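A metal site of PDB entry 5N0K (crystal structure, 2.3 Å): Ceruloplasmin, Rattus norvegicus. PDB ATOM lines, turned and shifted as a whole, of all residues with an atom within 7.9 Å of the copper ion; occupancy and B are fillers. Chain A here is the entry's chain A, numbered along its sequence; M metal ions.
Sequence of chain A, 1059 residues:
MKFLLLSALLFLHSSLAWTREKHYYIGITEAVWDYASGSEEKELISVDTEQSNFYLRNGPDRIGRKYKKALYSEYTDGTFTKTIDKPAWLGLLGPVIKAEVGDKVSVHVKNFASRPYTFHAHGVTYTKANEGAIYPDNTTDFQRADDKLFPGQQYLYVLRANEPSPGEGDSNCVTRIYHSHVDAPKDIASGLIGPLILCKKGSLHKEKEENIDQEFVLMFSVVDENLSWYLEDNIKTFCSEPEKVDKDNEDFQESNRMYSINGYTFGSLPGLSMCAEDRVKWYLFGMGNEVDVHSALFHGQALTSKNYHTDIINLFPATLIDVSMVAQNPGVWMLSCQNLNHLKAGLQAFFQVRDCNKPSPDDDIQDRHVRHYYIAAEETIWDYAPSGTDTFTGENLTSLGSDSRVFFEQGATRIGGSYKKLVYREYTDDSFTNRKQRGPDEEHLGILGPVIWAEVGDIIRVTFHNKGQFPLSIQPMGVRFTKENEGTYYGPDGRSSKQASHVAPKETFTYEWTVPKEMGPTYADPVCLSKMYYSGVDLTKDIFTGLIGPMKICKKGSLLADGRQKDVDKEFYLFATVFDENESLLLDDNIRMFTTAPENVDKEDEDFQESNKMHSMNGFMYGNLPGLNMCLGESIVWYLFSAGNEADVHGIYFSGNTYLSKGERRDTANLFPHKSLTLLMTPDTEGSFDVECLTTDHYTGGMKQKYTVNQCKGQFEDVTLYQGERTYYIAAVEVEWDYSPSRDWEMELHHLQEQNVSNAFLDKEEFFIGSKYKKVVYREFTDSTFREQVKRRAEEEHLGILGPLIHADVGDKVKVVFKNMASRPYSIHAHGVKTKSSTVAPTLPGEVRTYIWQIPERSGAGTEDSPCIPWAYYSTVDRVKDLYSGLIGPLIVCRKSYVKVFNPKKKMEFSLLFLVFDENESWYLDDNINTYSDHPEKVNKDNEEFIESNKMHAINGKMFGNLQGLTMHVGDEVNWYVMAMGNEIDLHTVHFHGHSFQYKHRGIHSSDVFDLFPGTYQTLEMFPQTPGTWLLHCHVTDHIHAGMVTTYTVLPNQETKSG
The side-chain amide nitrogen (ND2) of Asn 339 is in hydrogen-bond range of a ring nitrogen (NE2) of His 342, at 3.1 Å.
SG of Cys 337 sits close to N of Ser 295, 3.3 Å away.
The side-chain sulfur (SG) of Cys 337 lies close to the backbone NH (N) of Asn 339 (3.5 Å).
A ring nitrogen (NE2) of His 342 lies within hydrogen-bond range of the backbone carbonyl oxygen of Val 291, 2.9 Å away.
A ring nitrogen (NE2) of His 294 sits at hydrogen-bond distance from the side-chain carboxylate (OD2) of Asp 292 (2.8 Å).
The backbone NH (N) of Cys 337 sits at hydrogen-bond distance from the backbone carbonyl oxygen (O) of Leu 347, 3.2 Å away.
The side-chain carboxylate of Glu 646 is in hydrogen-bond range of a ring nitrogen (NE2) of His 342 (3.3 Å).
O of His 342 lies within hydrogen-bond range of N of Leu 347, at 3.1 Å.
The copper ion is bound by SG of Cys 337 (2.1 Å), ND1 of His 294 (2.1 Å) and ND1 of His 342 (2.2 Å).
The copper ion has three donor atoms within binding distance.
Residues that only touch the copper ion: Leu 347 and Val 293.
Within 4 Å of the copper ion: Val 293, His 294, Cys 337, His 342 and Leu 347.
The nearest printed residue that does not touch the copper ion is Asn 339 (4.1 Å).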
ATOM      1  N   PHE A 220     -11.631  13.887  13.954  1.00  0.00           N
ATOM      2  CA  PHE A 220     -12.404  14.633  14.933  1.00  0.00           C
ATOM      3  C   PHE A 220     -12.103  13.966  16.210  1.00  0.00           C
ATOM      4  O   PHE A 220     -12.313  12.775  16.332  1.00  0.00           O
ATOM      5  CB  PHE A 220     -13.923  14.592  14.666  1.00  0.00           C
ATOM      6  CG  PHE A 220     -14.390  15.606  13.639  1.00  0.00           C
ATOM      7  CD1 PHE A 220     -13.861  15.609  12.349  1.00  0.00           C
ATOM      8  CD2 PHE A 220     -15.320  16.577  13.965  1.00  0.00           C
ATOM      9  CE1 PHE A 220     -14.264  16.561  11.422  1.00  0.00           C
ATOM     10  CE2 PHE A 220     -15.735  17.511  13.033  1.00  0.00           C
ATOM     11  CZ  PHE A 220     -15.206  17.511  11.753  1.00  0.00           C
ATOM     12  N   SER A 221     -11.571  14.714  17.145  1.00  0.00           N
ATOM     13  CA  SER A 221     -11.193  14.152  18.402  1.00  0.00           C
ATOM     14  C   SER A 221     -11.170  15.186  19.534  1.00  0.00           C
ATOM     15  O   SER A 221     -10.711  16.312  19.334  1.00  0.00           O
ATOM     16  CB  SER A 221      -9.807  13.519  18.309  1.00  0.00           C
ATOM     17  OG  SER A 221      -9.538  12.775  19.492  1.00  0.00           O
ATOM     18  N   VAL A 222     -11.661  14.770  20.696  1.00  0.00           N
ATOM     19  CA  VAL A 222     -11.432  15.484  21.940  1.00  0.00           C
ATOM     20  C   VAL A 222     -10.087  14.952  22.451  1.00  0.00           C
ATOM     21  O   VAL A 222     -10.010  14.000  23.250  1.00  0.00           O
ATOM     22  CB  VAL A 222     -12.569  15.247  22.953  1.00  0.00           C
ATOM     23  CG1 VAL A 222     -12.316  16.032  24.238  1.00  0.00           C
ATOM     24  CG2 VAL A 222     -13.909  15.656  22.358  1.00  0.00           C
ATOM     25  N   TYR A 259     -10.751  20.167  21.878  1.00  0.00           N
ATOM     26  CA  TYR A 259     -11.819  19.683  20.998  1.00  0.00           C
ATOM     27  C   TYR A 259     -11.468  20.136  19.571  1.00  0.00           C
ATOM     28  O   TYR A 259     -11.735  21.276  19.196  1.00  0.00           O
ATOM     29  CB  TYR A 259     -13.179  20.230  21.411  1.00  0.00           C
ATOM     30  CG  TYR A 259     -13.730  19.749  22.750  1.00  0.00           C
ATOM     31  CD1 TYR A 259     -13.148  20.152  23.959  1.00  0.00           C
ATOM     32  CD2 TYR A 259     -14.885  18.966  22.822  1.00  0.00           C
ATOM     33  CE1 TYR A 259     -13.679  19.765  25.178  1.00  0.00           C
ATOM     34  CE2 TYR A 259     -15.416  18.569  24.038  1.00  0.00           C
ATOM     35  CZ  TYR A 259     -14.804  18.967  25.217  1.00  0.00           C
ATOM     36  OH  TYR A 259     -15.314  18.605  26.454  1.00  0.00           O
ATOM     37  N   SER A 260     -10.880  19.243  18.793  1.00  0.00           N
ATOM     38  CA  SER A 260     -10.111  19.614  17.622  1.00  0.00           C
ATOM     39  C   SER A 260     -10.362  18.739  16.407  1.00  0.00           C
ATOM     40  O   SER A 260     -10.896  17.641  16.518  1.00  0.00           O
ATOM     41  CB  SER A 260      -8.602  19.536  17.950  1.00  0.00           C
ATOM     42  OG  SER A 260      -8.255  18.400  18.723  1.00  0.00           O
ATOM     43  N   VAL A 291     -16.880  10.703  25.441  1.00  0.00           N
ATOM     44  CA  VAL A 291     -17.292  12.065  25.005  1.00  0.00           C
ATOM     45  C   VAL A 291     -17.164  12.273  23.492  1.00  0.00           C
ATOM     46  O   VAL A 291     -17.762  13.201  22.974  1.00  0.00           O
ATOM     47  CB  VAL A 291     -16.566  13.243  25.721  1.00  0.00           C
ATOM     48  CG1 VAL A 291     -17.051  13.367  27.149  1.00  0.00           C
ATOM     49  CG2 VAL A 291     -15.049  13.098  25.638  1.00  0.00           C
ATOM     50  N   ASP A 292     -16.427  11.420  22.804  1.00  0.00           N
ATOM     51  CA  ASP A 292     -16.277  11.529  21.349  1.00  0.00           C
ATOM     52  C   ASP A 292     -17.476  11.067  20.531  1.00  0.00           C
ATOM     53  O   ASP A 292     -17.385  10.095  19.762  1.00  0.00           O
ATOM     54  CB  ASP A 292     -14.996  10.824  20.923  1.00  0.00           C
ATOM     55  CG  ASP A 292     -13.759  11.580  21.406  1.00  0.00           C
ATOM     56  OD1 ASP A 292     -13.223  11.188  22.456  1.00  0.00           O
ATOM     57  OD2 ASP A 292     -13.386  12.582  20.755  1.00  0.00           O
ATOM     58  N   VAL A 293     -18.608  11.787  20.710  1.00  0.00           N
ATOM     59  CA  VAL A 293     -19.794  11.682  19.914  1.00  0.00           C
ATOM     60  C   VAL A 293     -19.741  12.906  19.038  1.00  0.00           C
ATOM     61  O   VAL A 293     -20.025  14.004  19.490  1.00  0.00           O
ATOM     62  CB  VAL A 293     -21.053  11.676  20.786  1.00  0.00           C
ATOM     63  CG1 VAL A 293     -22.313  11.644  19.923  1.00  0.00           C
ATOM     64  CG2 VAL A 293     -21.037  10.456  21.708  1.00  0.00           C
ATOM     65  N   HIS A 294     -19.336  12.719  17.786  1.00  0.00           N
ATOM     66  CA  HIS A 294     -19.178  13.828  16.853  1.00  0.00           C
ATOM     67  C   HIS A 294     -20.208  13.827  15.750  1.00  0.00           C
ATOM     68  O   HIS A 294     -20.684  12.774  15.327  1.00  0.00           O
ATOM     69  CB  HIS A 294     -17.787  13.808  16.208  1.00  0.00           C
ATOM     70  CG  HIS A 294     -16.673  13.813  17.202  1.00  0.00           C
ATOM     71  ND1 HIS A 294     -16.279  14.950  17.871  1.00  0.00           N
ATOM     72  CD2 HIS A 294     -15.878  12.813  17.679  1.00  0.00           C
ATOM     73  CE1 HIS A 294     -15.268  14.670  18.672  1.00  0.00           C
ATOM     74  NE2 HIS A 294     -15.017  13.372  18.591  1.00  0.00           N
ATOM     75  N   SER A 295     -20.508  15.039  15.268  1.00  0.00           N
ATOM     76  CA  SER A 295     -21.506  15.260  14.215  1.00  0.00           C
ATOM     77  C   SER A 295     -20.949  16.344  13.294  1.00  0.00           C
ATOM     78  O   SER A 295     -21.217  17.541  13.410  1.00  0.00           O
ATOM     79  CB  SER A 295     -22.811  15.695  14.880  1.00  0.00           C
ATOM     80  OG  SER A 295     -23.393  14.599  15.620  1.00  0.00           O
ATOM     81  N   ALA A 296     -20.117  15.911  12.369  1.00  0.00           N
ATOM     82  CA  ALA A 296     -19.520  16.807  11.370  1.00  0.00           C
ATOM     83  C   ALA A 296     -20.508  17.382  10.389  1.00  0.00           C
ATOM     84  O   ALA A 296     -21.187  16.621   9.691  1.00  0.00           O
ATOM     85  CB  ALA A 296     -18.432  16.078  10.607  1.00  0.00           C
ATOM     86  N   ILE A 313     -22.061  13.865   9.247  1.00  0.00           N
ATOM     87  CA  ILE A 313     -21.218  12.687   9.369  1.00  0.00           C
ATOM     88  C   ILE A 313     -20.913  12.474  10.849  1.00  0.00           C
ATOM     89  O   ILE A 313     -20.227  13.297  11.469  1.00  0.00           O
ATOM     90  CB  ILE A 313     -19.904  12.798   8.558  1.00  0.00           C
ATOM     91  CG1 ILE A 313     -20.191  12.783   7.040  1.00  0.00           C
ATOM     92  CG2 ILE A 313     -18.995  11.621   8.859  1.00  0.00           C
ATOM     93  CD1 ILE A 313     -20.529  14.151   6.484  1.00  0.00           C
ATOM     94  N   LEU A 315     -19.188  10.451  13.966  1.00  0.00           N
ATOM     95  CA  LEU A 315     -17.868   9.848  14.127  1.00  0.00           C
ATOM     96  C   LEU A 315     -17.729   9.548  15.576  1.00  0.00           C
ATOM     97  O   LEU A 315     -18.061  10.376  16.389  1.00  0.00           O
ATOM     98  CB  LEU A 315     -16.752  10.806  13.716  1.00  0.00           C
ATOM     99  CG  LEU A 315     -16.752  11.238  12.246  1.00  0.00           C
ATOM    100  CD1 LEU A 315     -15.803  12.372  12.070  1.00  0.00           C
ATOM    101  CD2 LEU A 315     -16.426  10.099  11.278  1.00  0.00           C
ATOM    102  N   SER A 336     -18.008  22.285  11.338  1.00  0.00           N
ATOM    103  CA  SER A 336     -18.192  22.256  12.771  1.00  0.00           C
ATOM    104  C   SER A 336     -18.742  20.901  13.228  1.00  0.00           C
ATOM    105  O   SER A 336     -19.259  20.136  12.434  1.00  0.00           O
ATOM    106  CB  SER A 336     -19.178  23.333  13.175  1.00  0.00           C
ATOM    107  OG  SER A 336     -20.382  23.143  12.469  1.00  0.00           O
ATOM    108  N   CYS A 337     -18.548  20.596  14.492  1.00  0.00           N
ATOM    109  CA  CYS A 337     -19.248  19.491  15.131  1.00  0.00           C
ATOM    110  C   CYS A 337     -20.521  20.088  15.727  1.00  0.00           C
ATOM    111  O   CYS A 337     -20.468  21.081  16.425  1.00  0.00           O
ATOM    112  CB  CYS A 337     -18.368  18.840  16.191  1.00  0.00           C
ATOM    113  SG  CYS A 337     -19.180  17.512  17.067  1.00  0.00           S
ATOM    114  N   GLN A 338     -21.664  19.472  15.440  1.00  0.00           N
ATOM    115  CA  GLN A 338     -22.954  19.915  15.953  1.00  0.00           C
ATOM    116  C   GLN A 338     -23.342  19.316  17.278  1.00  0.00           C
ATOM    117  O   GLN A 338     -24.433  19.567  17.770  1.00  0.00           O
ATOM    118  CB  GLN A 338     -24.037  19.607  14.922  1.00  0.00           C
ATOM    119  CG  GLN A 338     -23.843  20.312  13.594  1.00  0.00           C
ATOM    120  CD  GLN A 338     -24.032  21.812  13.722  1.00  0.00           C
ATOM    121  OE1 GLN A 338     -25.152  22.309  13.687  1.00  0.00           O
ATOM    122  NE2 GLN A 338     -22.958  22.522  13.865  1.00  0.00           N
ATOM    123  N   ASN A 339     -22.480  18.473  17.851  1.00  0.00           N
ATOM    124  CA  ASN A 339     -22.551  18.160  19.277  1.00  0.00           C
ATOM    125  C   ASN A 339     -22.376  19.510  19.971  1.00  0.00           C
ATOM    126  O   ASN A 339     -21.287  20.073  19.963  1.00  0.00           O
ATOM    127  CB  ASN A 339     -21.463  17.188  19.703  1.00  0.00           C
ATOM    128  CG  ASN A 339     -21.422  16.943  21.203  1.00  0.00           C
ATOM    129  OD1 ASN A 339     -21.710  17.824  22.001  1.00  0.00           O
ATOM    130  ND2 ASN A 339     -21.030  15.719  21.592  1.00  0.00           N
ATOM    131  N   LEU A 340     -23.475  19.991  20.575  1.00  0.00           N
ATOM    132  CA  LEU A 340     -23.526  21.337  21.134  1.00  0.00           C
ATOM    133  C   LEU A 340     -22.460  21.580  22.220  1.00  0.00           C
ATOM    134  O   LEU A 340     -21.930  22.707  22.313  1.00  0.00           O
ATOM    135  CB  LEU A 340     -24.909  21.606  21.701  1.00  0.00           C
ATOM    136  CG  LEU A 340     -26.036  21.539  20.669  1.00  0.00           C
ATOM    137  CD1 LEU A 340     -27.331  21.841  21.403  1.00  0.00           C
ATOM    138  CD2 LEU A 340     -25.803  22.450  19.491  1.00  0.00           C
ATOM    139  N   ASN A 341     -22.117  20.555  23.001  1.00  0.00           N
ATOM    140  CA  ASN A 341     -20.982  20.684  23.915  1.00  0.00           C
ATOM    141  C   ASN A 341     -19.650  20.834  23.229  1.00  0.00           C
ATOM    142  O   ASN A 341     -18.806  21.565  23.730  1.00  0.00           O
ATOM    143  CB  ASN A 341     -20.893  19.539  24.891  1.00  0.00           C
ATOM    144  CG  ASN A 341     -21.942  19.626  25.994  1.00  0.00           C
ATOM    145  OD1 ASN A 341     -22.596  20.627  26.186  1.00  0.00           O
ATOM    146  ND2 ASN A 341     -22.131  18.542  26.683  1.00  0.00           N
ATOM    147  N   HIS A 342     -19.469  20.160  22.098  1.00  0.00           N
ATOM    148  CA  HIS A 342     -18.230  20.227  21.354  1.00  0.00           C
ATOM    149  C   HIS A 342     -18.055  21.531  20.619  1.00  0.00           C
ATOM    150  O   HIS A 342     -16.957  22.075  20.564  1.00  0.00           O
ATOM    151  CB  HIS A 342     -18.125  19.063  20.370  1.00  0.00           C
ATOM    152  CG  HIS A 342     -18.008  17.733  21.019  1.00  0.00           C
ATOM    153  ND1 HIS A 342     -17.547  16.640  20.359  1.00  0.00           N
ATOM    154  CD2 HIS A 342     -18.301  17.333  22.277  1.00  0.00           C
ATOM    155  CE1 HIS A 342     -17.587  15.590  21.157  1.00  0.00           C
ATOM    156  NE2 HIS A 342     -18.007  15.986  22.329  1.00  0.00           N
ATOM    157  N   LEU A 343     -19.150  22.017  20.034  1.00  0.00           N
ATOM    158  CA  LEU A 343     -19.170  23.254  19.282  1.00  0.00           C
ATOM    159  C   LEU A 343     -18.700  24.413  20.126  1.00  0.00           C
ATOM    160  O   LEU A 343     -17.782  25.116  19.743  1.00  0.00           O
ATOM    161  CB  LEU A 343     -20.582  23.523  18.802  1.00  0.00           C
ATOM    162  CG  LEU A 343     -20.792  24.697  17.900  1.00  0.00           C
ATOM    163  CD1 LEU A 343     -20.188  24.442  16.546  1.00  0.00           C
ATOM    164  CD2 LEU A 343     -22.283  24.825  17.731  1.00  0.00           C
ATOM    165  N   LEU A 347     -14.680  23.123  18.677  1.00  0.00           N
ATOM    166  CA  LEU A 347     -14.539  22.155  17.570  1.00  0.00           C
ATOM    167  C   LEU A 347     -15.211  22.661  16.275  1.00  0.00           C
ATOM    168  O   LEU A 347     -16.383  22.368  15.947  1.00  0.00           O
ATOM    169  CB  LEU A 347     -15.077  20.805  17.966  1.00  0.00           C
ATOM    170  CG  LEU A 347     -14.332  19.635  17.341  1.00  0.00           C
ATOM    171  CD1 LEU A 347     -14.931  18.387  17.989  1.00  0.00           C
ATOM    172  CD2 LEU A 347     -14.467  19.634  15.813  1.00  0.00           C
ATOM    173  N   GLU A 646     -23.362  14.826  23.652  1.00  0.00           N
ATOM    174  CA  GLU A 646     -22.974  13.421  23.786  1.00  0.00           C
ATOM    175  C   GLU A 646     -23.966  12.527  24.551  1.00  0.00           C
ATOM    176  O   GLU A 646     -23.958  11.299  24.373  1.00  0.00           O
ATOM    177  CB  GLU A 646     -21.555  13.282  24.322  1.00  0.00           C
ATOM    178  CG  GLU A 646     -21.276  13.893  25.707  1.00  0.00           C
ATOM    179  CD  GLU A 646     -20.920  15.383  25.680  1.00  0.00           C
ATOM    180  OE1 GLU A 646     -20.355  15.926  24.690  1.00  0.00           O
ATOM    181  OE2 GLU A 646     -21.229  16.025  26.684  1.00  0.00           O
HETATM  182 CU    CU M   1     -17.680  16.546  18.165  1.00  0.00          CU
